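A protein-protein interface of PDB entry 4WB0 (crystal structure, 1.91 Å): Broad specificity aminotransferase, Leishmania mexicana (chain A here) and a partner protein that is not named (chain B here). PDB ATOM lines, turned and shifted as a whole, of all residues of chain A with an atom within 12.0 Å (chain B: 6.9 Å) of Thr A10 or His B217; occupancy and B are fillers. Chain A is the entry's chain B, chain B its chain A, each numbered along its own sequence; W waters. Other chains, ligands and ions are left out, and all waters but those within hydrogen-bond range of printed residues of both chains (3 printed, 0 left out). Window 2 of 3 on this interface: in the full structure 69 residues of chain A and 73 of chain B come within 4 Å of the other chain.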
ATOM      1  N   ALA A   7       3.791  24.767   5.438  1.00  0.00           N
ATOM      2  CA  ALA A   7       4.051  24.267   4.082  1.00  0.00           C
ATOM      3  C   ALA A   7       3.736  22.765   3.942  1.00  0.00           C
ATOM      4  O   ALA A   7       4.460  21.903   4.455  1.00  0.00           O
ATOM      5  CB  ALA A   7       5.506  24.539   3.701  1.00  0.00           C
ATOM      6  N   ALA A   8       2.665  22.449   3.224  1.00  0.00           N
ATOM      7  CA  ALA A   8       2.295  21.062   2.953  1.00  0.00           C
ATOM      8  C   ALA A   8       3.459  20.315   2.321  1.00  0.00           C
ATOM      9  O   ALA A   8       4.220  20.883   1.546  1.00  0.00           O
ATOM     10  CB  ALA A   8       1.063  20.995   2.043  1.00  0.00           C
ATOM     11  N   MET A   9       3.592  19.036   2.660  1.00  0.00           N
ATOM     12  CA  MET A   9       4.657  18.211   2.131  1.00  0.00           C
ATOM     13  C   MET A   9       4.104  16.922   1.510  1.00  0.00           C
ATOM     14  O   MET A   9       4.363  16.636   0.340  1.00  0.00           O
ATOM     15  CB  MET A   9       5.651  17.864   3.222  1.00  0.00           C
ATOM     16  CG  MET A   9       6.895  17.288   2.681  1.00  0.00           C
ATOM     17  SD  MET A   9       8.196  17.227   3.931  1.00  0.00           S
ATOM     18  CE  MET A   9       8.731  18.930   4.097  1.00  0.00           C
ATOM     19  N   THR A  10       3.377  16.145   2.303  1.00  0.00           N
ATOM     20  CA  THR A  10       2.785  14.905   1.784  1.00  0.00           C
ATOM     21  C   THR A  10       1.534  15.189   0.957  1.00  0.00           C
ATOM     22  O   THR A  10       0.981  16.263   1.025  1.00  0.00           O
ATOM     23  CB  THR A  10       2.423  13.963   2.919  1.00  0.00           C
ATOM     24  OG1 THR A  10       1.425  14.592   3.736  1.00  0.00           O
ATOM     25  CG2 THR A  10       3.685  13.670   3.809  1.00  0.00           C
ATOM     26  N   THR A  11       1.063  14.219   0.178  1.00  0.00           N
ATOM     27  CA  THR A  11      -0.106  14.499  -0.667  1.00  0.00           C
ATOM     28  C   THR A  11      -1.298  14.773   0.233  1.00  0.00           C
ATOM     29  O   THR A  11      -2.116  15.640  -0.055  1.00  0.00           O
ATOM     30  CB  THR A  11      -0.448  13.350  -1.633  1.00  0.00           C
ATOM     31  OG1 THR A  11      -0.523  12.115  -0.930  1.00  0.00           O
ATOM     32  CG2 THR A  11       0.606  13.247  -2.710  1.00  0.00           C
ATOM     33  N   THR A  12      -1.384  14.064   1.348  1.00  0.00           N
ATOM     34  CA  THR A  12      -2.561  14.229   2.210  1.00  0.00           C
ATOM     35  C   THR A  12      -2.628  15.671   2.757  1.00  0.00           C
ATOM     36  O   THR A  12      -3.713  16.261   2.907  1.00  0.00           O
ATOM     37  CB  THR A  12      -2.574  13.227   3.362  1.00  0.00           C
ATOM     38  OG1 THR A  12      -3.812  13.374   4.090  1.00  0.00           O
ATOM     39  CG2 THR A  12      -1.432  13.459   4.294  1.00  0.00           C
ATOM     40  N   GLU A  13      -1.462  16.240   3.003  1.00  0.00           N
ATOM     41  CA  GLU A  13      -1.358  17.629   3.470  1.00  0.00           C
ATOM     42  C   GLU A  13      -1.739  18.595   2.362  1.00  0.00           C
ATOM     43  O   GLU A  13      -2.357  19.603   2.620  1.00  0.00           O
ATOM     44  CB  GLU A  13       0.064  17.925   3.987  1.00  0.00           C
ATOM     45  CG  GLU A  13       0.318  17.333   5.396  1.00  0.00           C
ATOM     46  CD  GLU A  13       1.782  17.391   5.830  1.00  0.00           C
ATOM     47  OE1 GLU A  13       2.666  17.563   4.951  1.00  0.00           O
ATOM     48  OE2 GLU A  13       2.057  17.234   7.053  1.00  0.00           O
ATOM     49  N   ARG A  14      -1.368  18.303   1.129  1.00  0.00           N
ATOM     50  CA  ARG A  14      -1.830  19.140  -0.012  1.00  0.00           C
ATOM     51  C   ARG A  14      -3.335  19.060  -0.229  1.00  0.00           C
ATOM     52  O   ARG A  14      -3.985  20.081  -0.360  1.00  0.00           O
ATOM     53  CB  ARG A  14      -1.111  18.766  -1.318  1.00  0.00           C
ATOM     54  CG  ARG A  14       0.413  19.094  -1.270  1.00  0.00           C
ATOM     55  CD  ARG A  14       1.097  18.793  -2.581  1.00  0.00           C
ATOM     56  NE  ARG A  14       2.548  18.727  -2.505  1.00  0.00           N
ATOM     57  CZ  ARG A  14       3.339  19.770  -2.278  1.00  0.00           C
ATOM     58  NH1 ARG A  14       2.823  20.991  -2.095  1.00  0.00           N
ATOM     59  NH2 ARG A  14       4.650  19.586  -2.223  1.00  0.00           N
ATOM     60  N   TRP A  15      -3.902  17.866  -0.252  1.00  0.00           N
ATOM     61  CA  TRP A  15      -5.352  17.748  -0.370  1.00  0.00           C
ATOM     62  C   TRP A  15      -6.034  18.464   0.796  1.00  0.00           C
ATOM     63  O   TRP A  15      -7.090  19.058   0.612  1.00  0.00           O
ATOM     64  CB  TRP A  15      -5.783  16.286  -0.434  1.00  0.00           C
ATOM     65  CG  TRP A  15      -5.437  15.713  -1.767  1.00  0.00           C
ATOM     66  CD1 TRP A  15      -4.407  14.893  -2.055  1.00  0.00           C
ATOM     67  CD2 TRP A  15      -6.146  15.934  -2.996  1.00  0.00           C
ATOM     68  NE1 TRP A  15      -4.404  14.594  -3.426  1.00  0.00           N
ATOM     69  CE2 TRP A  15      -5.450  15.244  -4.015  1.00  0.00           C
ATOM     70  CE3 TRP A  15      -7.306  16.654  -3.335  1.00  0.00           C
ATOM     71  CZ2 TRP A  15      -5.868  15.250  -5.353  1.00  0.00           C
ATOM     72  CZ3 TRP A  15      -7.707  16.690  -4.673  1.00  0.00           C
ATOM     73  CH2 TRP A  15      -7.000  15.972  -5.662  1.00  0.00           C
ATOM     74  N   GLN A  16      -5.404  18.445   1.985  1.00  0.00           N
ATOM     75  CA  GLN A  16      -5.978  19.140   3.139  1.00  0.00           C
ATOM     76  C   GLN A  16      -6.203  20.603   2.890  1.00  0.00           C
ATOM     77  O   GLN A  16      -7.137  21.192   3.440  1.00  0.00           O
ATOM     78  CB  GLN A  16      -5.076  19.016   4.373  1.00  0.00           C
ATOM     79  CG  GLN A  16      -5.144  17.685   4.983  1.00  0.00           C
ATOM     80  CD  GLN A  16      -6.098  17.585   6.144  1.00  0.00           C
ATOM     81  OE1 GLN A  16      -7.023  18.414   6.327  1.00  0.00           O
ATOM     82  NE2 GLN A  16      -5.842  16.572   6.993  1.00  0.00           N
ATOM     83  N   LYS A  17      -5.318  21.203   2.113  1.00  0.00           N
ATOM     84  CA  LYS A  17      -5.411  22.621   1.850  1.00  0.00           C
ATOM     85  C   LYS A  17      -6.365  23.000   0.721  1.00  0.00           C
ATOM     86  O   LYS A  17      -6.574  24.185   0.467  1.00  0.00           O
ATOM     87  CB  LYS A  17      -4.021  23.176   1.557  1.00  0.00           C
ATOM     88  CG  LYS A  17      -3.136  23.257   2.832  1.00  0.00           C
ATOM     89  CD  LYS A  17      -1.868  24.045   2.599  1.00  0.00           C
ATOM     90  CE  LYS A  17      -0.963  24.020   3.841  1.00  0.00           C
ATOM     91  NZ  LYS A  17       0.384  24.643   3.616  1.00  0.00           N
ATOM     92  N   ILE A  18      -6.977  22.038   0.056  1.00  0.00           N
ATOM     93  CA  ILE A  18      -7.905  22.439  -1.035  1.00  0.00           C
ATOM     94  C   ILE A  18      -9.088  23.292  -0.514  1.00  0.00           C
ATOM     95  O   ILE A  18      -9.713  22.982   0.516  1.00  0.00           O
ATOM     96  CB  ILE A  18      -8.432  21.212  -1.792  1.00  0.00           C
ATOM     97  CG1 ILE A  18      -8.898  21.593  -3.199  1.00  0.00           C
ATOM     98  CG2 ILE A  18      -9.566  20.520  -1.038  1.00  0.00           C
ATOM     99  CD1 ILE A  18      -9.513  20.404  -4.029  1.00  0.00           C
ATOM    100  N   PHE B 127      -2.126  21.520  -6.426  1.00  0.00           N
ATOM    101  CA  PHE B 127      -0.712  21.726  -6.810  1.00  0.00           C
ATOM    102  C   PHE B 127      -0.593  22.980  -7.616  1.00  0.00           C
ATOM    103  O   PHE B 127      -1.557  23.391  -8.274  1.00  0.00           O
ATOM    104  CB  PHE B 127      -0.197  20.518  -7.650  1.00  0.00           C
ATOM    105  CG  PHE B 127      -0.165  19.236  -6.890  1.00  0.00           C
ATOM    106  CD1 PHE B 127      -1.302  18.486  -6.743  1.00  0.00           C
ATOM    107  CD2 PHE B 127       0.996  18.791  -6.289  1.00  0.00           C
ATOM    108  CE1 PHE B 127      -1.286  17.299  -6.007  1.00  0.00           C
ATOM    109  CE2 PHE B 127       0.999  17.590  -5.566  1.00  0.00           C
ATOM    110  CZ  PHE B 127      -0.117  16.865  -5.439  1.00  0.00           C
ATOM    111  N   PRO B 182      11.515  16.507  -8.668  1.00  0.00           N
ATOM    112  CA  PRO B 182      11.293  17.190  -7.385  1.00  0.00           C
ATOM    113  C   PRO B 182      10.173  16.532  -6.596  1.00  0.00           C
ATOM    114  O   PRO B 182       9.219  15.995  -7.194  1.00  0.00           O
ATOM    115  CB  PRO B 182      10.910  18.625  -7.791  1.00  0.00           C
ATOM    116  CG  PRO B 182      10.451  18.515  -9.217  1.00  0.00           C
ATOM    117  CD  PRO B 182      11.221  17.387  -9.819  1.00  0.00           C
ATOM    118  N   ASP B 183      10.292  16.550  -5.272  1.00  0.00           N
ATOM    119  CA  ASP B 183       9.251  15.947  -4.441  1.00  0.00           C
ATOM    120  C   ASP B 183       7.917  16.562  -4.771  1.00  0.00           C
ATOM    121  O   ASP B 183       7.838  17.747  -5.041  1.00  0.00           O
ATOM    122  CB  ASP B 183       9.506  16.166  -2.964  1.00  0.00           C
ATOM    123  CG  ASP B 183      10.532  15.201  -2.366  1.00  0.00           C
ATOM    124  OD1 ASP B 183      11.284  14.530  -3.125  1.00  0.00           O
ATOM    125  OD2 ASP B 183      10.581  15.149  -1.095  1.00  0.00           O
ATOM    126  N   GLY B 184       6.858  15.763  -4.769  1.00  0.00           N
ATOM    127  CA  GLY B 184       5.545  16.333  -4.819  1.00  0.00           C
ATOM    128  C   GLY B 184       5.147  16.704  -6.234  1.00  0.00           C
ATOM    129  O   GLY B 184       4.356  17.630  -6.441  1.00  0.00           O
ATOM    130  N   SER B 185       5.689  15.965  -7.192  1.00  0.00           N
ATOM    131  CA  SER B 185       5.296  16.062  -8.571  1.00  0.00           C
ATOM    132  C   SER B 185       4.111  15.126  -8.864  1.00  0.00           C
ATOM    133  O   SER B 185       3.760  14.261  -8.032  1.00  0.00           O
ATOM    134  CB  SER B 185       6.465  15.686  -9.479  1.00  0.00           C
ATOM    135  OG  SER B 185       7.557  16.582  -9.347  1.00  0.00           O
ATOM    136  N   LEU B 212       8.584   4.223  -4.134  1.00  0.00           N
ATOM    137  CA  LEU B 212       9.236   5.464  -4.596  1.00  0.00           C
ATOM    138  C   LEU B 212       8.275   6.627  -4.609  1.00  0.00           C
ATOM    139  O   LEU B 212       8.647   7.724  -4.253  1.00  0.00           O
ATOM    140  CB  LEU B 212       9.822   5.307  -5.995  1.00  0.00           C
ATOM    141  CG  LEU B 212      10.949   4.274  -6.117  1.00  0.00           C
ATOM    142  CD1 LEU B 212      11.309   4.114  -7.601  1.00  0.00           C
ATOM    143  CD2 LEU B 212      12.159   4.704  -5.346  1.00  0.00           C
ATOM    144  N   MET B 213       7.032   6.371  -5.036  1.00  0.00           N
ATOM    145  CA  MET B 213       6.039   7.416  -5.054  1.00  0.00           C
ATOM    146  C   MET B 213       5.819   7.896  -3.609  1.00  0.00           C
ATOM    147  O   MET B 213       5.703   9.093  -3.355  1.00  0.00           O
ATOM    148  CB  MET B 213       4.722   6.939  -5.676  1.00  0.00           C
ATOM    149  CG  MET B 213       4.821   6.625  -7.157  1.00  0.00           C
ATOM    150  SD  MET B 213       5.135   8.102  -8.159  1.00  0.00           S
ATOM    151  CE  MET B 213       5.586   7.405  -9.732  1.00  0.00           C
ATOM    152  N   LEU B 214       5.758   6.958  -2.671  1.00  0.00           N
ATOM    153  CA  LEU B 214       5.584   7.326  -1.272  1.00  0.00           C
ATOM    154  C   LEU B 214       6.751   8.155  -0.748  1.00  0.00           C
ATOM    155  O   LEU B 214       6.572   9.186  -0.077  1.00  0.00           O
ATOM    156  CB  LEU B 214       5.439   6.085  -0.401  1.00  0.00           C
ATOM    157  CG  LEU B 214       4.085   5.435  -0.554  1.00  0.00           C
ATOM    158  CD1 LEU B 214       4.126   4.139   0.096  1.00  0.00           C
ATOM    159  CD2 LEU B 214       2.994   6.318   0.037  1.00  0.00           C
ATOM    160  N   ALA B 215       7.960   7.684  -1.011  1.00  0.00           N
ATOM    161  CA  ALA B 215       9.132   8.369  -0.467  1.00  0.00           C
ATOM    162  C   ALA B 215       9.363   9.764  -1.057  1.00  0.00           C
ATOM    163  O   ALA B 215      10.059  10.546  -0.455  1.00  0.00           O
ATOM    164  CB  ALA B 215      10.349   7.553  -0.683  1.00  0.00           C
ATOM    165  N   LYS B 216       8.877  10.028  -2.266  1.00  0.00           N
ATOM    166  CA  LYS B 216       9.042  11.327  -2.898  1.00  0.00           C
ATOM    167  C   LYS B 216       7.815  12.240  -2.744  1.00  0.00           C
ATOM    168  O   LYS B 216       7.797  13.336  -3.298  1.00  0.00           O
ATOM    169  CB  LYS B 216       9.313  11.135  -4.392  1.00  0.00           C
ATOM    170  CG  LYS B 216      10.602  10.435  -4.738  1.00  0.00           C
ATOM    171  CD  LYS B 216      11.800  11.315  -4.614  1.00  0.00           C
ATOM    172  CE  LYS B 216      11.688  12.512  -5.576  1.00  0.00           C
ATOM    173  NZ  LYS B 216      12.901  13.357  -5.430  1.00  0.00           N
ATOM    174  N   HIS B 217       6.775  11.744  -2.081  1.00  0.00           N
ATOM    175  CA  HIS B 217       5.516  12.481  -1.886  1.00  0.00           C
ATOM    176  C   HIS B 217       4.877  12.859  -3.207  1.00  0.00           C
ATOM    177  O   HIS B 217       4.138  13.859  -3.288  1.00  0.00           O
ATOM    178  CB  HIS B 217       5.703  13.736  -1.070  1.00  0.00           C
ATOM    179  CG  HIS B 217       6.561  13.570   0.143  1.00  0.00           C
ATOM    180  ND1 HIS B 217       6.228  12.735   1.182  1.00  0.00           N
ATOM    181  CD2 HIS B 217       7.719  14.182   0.497  1.00  0.00           C
ATOM    182  CE1 HIS B 217       7.169  12.801   2.111  1.00  0.00           C
ATOM    183  NE2 HIS B 217       8.090  13.662   1.717  1.00  0.00           N
ATOM    184  N   HIS B 218       5.042  12.005  -4.225  1.00  0.00           N
ATOM    185  CA  HIS B 218       4.433  12.264  -5.519  1.00  0.00           C
ATOM    186  C   HIS B 218       2.923  11.984  -5.519  1.00  0.00           C
ATOM    187  O   HIS B 218       2.404  11.115  -4.762  1.00  0.00           O
ATOM    188  CB  HIS B 218       5.064  11.416  -6.632  1.00  0.00           C
ATOM    189  CG  HIS B 218       6.472  11.819  -6.987  1.00  0.00           C
ATOM    190  ND1 HIS B 218       6.904  13.122  -6.957  1.00  0.00           N
ATOM    191  CD2 HIS B 218       7.529  11.074  -7.406  1.00  0.00           C
ATOM    192  CE1 HIS B 218       8.185  13.159  -7.305  1.00  0.00           C
ATOM    193  NE2 HIS B 218       8.583  11.936  -7.586  1.00  0.00           N
ATOM    194  N   GLN B 219       2.221  12.677  -6.417  1.00  0.00           N
ATOM    195  CA  GLN B 219       0.825  12.386  -6.659  1.00  0.00           C
ATOM    196  C   GLN B 219       0.690  11.432  -7.826  1.00  0.00           C
ATOM    197  O   GLN B 219       1.204  11.715  -8.908  1.00  0.00           O
ATOM    198  CB  GLN B 219       0.057  13.678  -6.952  1.00  0.00           C
ATOM    199  CG  GLN B 219      -1.390  13.474  -7.433  1.00  0.00           C
ATOM    200  CD  GLN B 219      -2.326  13.054  -6.294  1.00  0.00           C
ATOM    201  OE1 GLN B 219      -2.306  13.632  -5.184  1.00  0.00           O
ATOM    202  NE2 GLN B 219      -3.147  12.024  -6.559  1.00  0.00           N
ATOM    203  N   GLU B 250      -2.757   8.111  -2.204  1.00  0.00           N
ATOM    204  CA  GLU B 250      -3.975   8.874  -2.537  1.00  0.00           C
ATOM    205  C   GLU B 250      -4.147   8.926  -4.033  1.00  0.00           C
ATOM    206  O   GLU B 250      -3.911   9.954  -4.684  1.00  0.00           O
ATOM    207  CB  GLU B 250      -3.912  10.269  -1.950  1.00  0.00           C
ATOM    208  CG  GLU B 250      -4.088  10.257  -0.439  1.00  0.00           C
ATOM    209  CD  GLU B 250      -4.136  11.676   0.116  1.00  0.00           C
ATOM    210  OE1 GLU B 250      -3.080  12.340   0.067  1.00  0.00           O
ATOM    211  OE2 GLU B 250      -5.225  12.127   0.568  1.00  0.00           O
HETATM  212  O   HOH W   1       4.264  20.187  -5.492  1.00  0.00           O
HETATM  213  O   HOH W   2      -0.118   9.735  -2.171  1.00  0.00           O
HETATM  214  O   HOH W   3       3.027  15.936  -2.056  1.00  0.00           O
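Among the printed residues, merely in contact across the chains: Met A9 with His B217 (3.5 Å), Thr A10 with His B217 (3.8 Å), Thr A11 with His B217 (3.6 Å), Thr A11 with His B218 (3.5 Å), Thr A11 with Gln B219 (3.8 Å), Arg A14 with Phe B127 (3.2 Å) and Trp A15 with Glu B250 (3.6 Å).
Thr A10 touches just one residue of chain B: His B217 (3.8 Å).
His B217 touches just these residues of chain A: Met A9, Thr A10 and Thr A11.
No residue of chain A comes within 4 Å of Asp B183.
No residue of chain A comes within 4 Å of Gly B184.
No residue of chain A comes within 4 Å of Ser B185.
No residue of chain A comes within 4 Å of Ala B215.
No residue of chain A comes within 4 Å of Lys B216.
Of chain A, only Thr A11 (3.5 Å) comes within 4 Å of His B218.
Printed residues of chain B within 4 Å of Trp A15: Gln B219 (2.9 Å) and Glu B250 (3.6 Å).
Of the printed residues of chain A, Phe B127 touches Arg A14.
Of the printed residues of chain B, Thr A12 touches Glu B250 (2.7 Å).
Printed residues of chain A within 4 Å of Glu B250: Thr A11 (2.8 Å), Thr A12 (2.7 Å) and Trp A15 (3.6 Å).
Ala A8 touches none of the printed residues of chain B.
Gln A16 touches none of the printed residues of chain B.
The nearest residue of chain B that does not touch Thr A10 is Glu B250 (5.5 Å).
The nearest residue of chain A that does not touch His B217 is Arg A14 (5.2 Å).
N of Gly B184 sits at hydrogen-bond distance from ND1 of His B218, 3.4 Å away.
A ring nitrogen (ND1) of His B218 is in hydrogen-bond range of the backbone NH (N) of Ser B185, at 3.1 Å.
N of Gln B219 sits at hydrogen-bond distance from O of Ser B185, at 2.7 Å.
The backbone carbonyl oxygen (O) of Met B213 is in hydrogen-bond range of the backbone NH (N) of His B218 (3.1 Å).
The backbone carbonyl oxygen (O) of Glu B250 lies within hydrogen-bond range of the side-chain amide nitrogen (NE2) of Gln B219 (2.9 Å).
N of Thr A10 lies within hydrogen-bond range of OE1 of Glu A13 (3.1 Å).
Hydrophobic or aromatic side chains of chain B that line the printed part of chain A: Phe B127 and His B217.
Among the printed residues, no Asp or Glu carboxylate lies within 4 Å of a Lys or Arg side-chain nitrogen of the other chain.
The indole nitrogen (NE1) of Trp A15 lies within hydrogen-bond range of the side-chain amide oxygen (OE1) of Gln B219 (2.9 Å).
OE1 of Glu B250 is in hydrogen-bond range of OG1 of Thr A11, 2.8 Å away.
The backbone NH of Thr A12 sits at hydrogen-bond distance from the side-chain carboxylate of Glu B250 (2.7 Å).
Water W3 lies within hydrogen-bond range of O of His B217 (2.7 Å), O of Met A9 (2.8 Å), NE of Arg A14 (2.9 Å) and N of Thr A11 (3.4 Å).
Water W2 bridges OG1 of Thr A11 and N of Glu B250.
Water W1 lies within hydrogen-bond range of the backbone carbonyl oxygen (O) of Gly B184 (2.7 Å) and the guanidinium group (NH2) of Arg A14 (3.3 Å).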
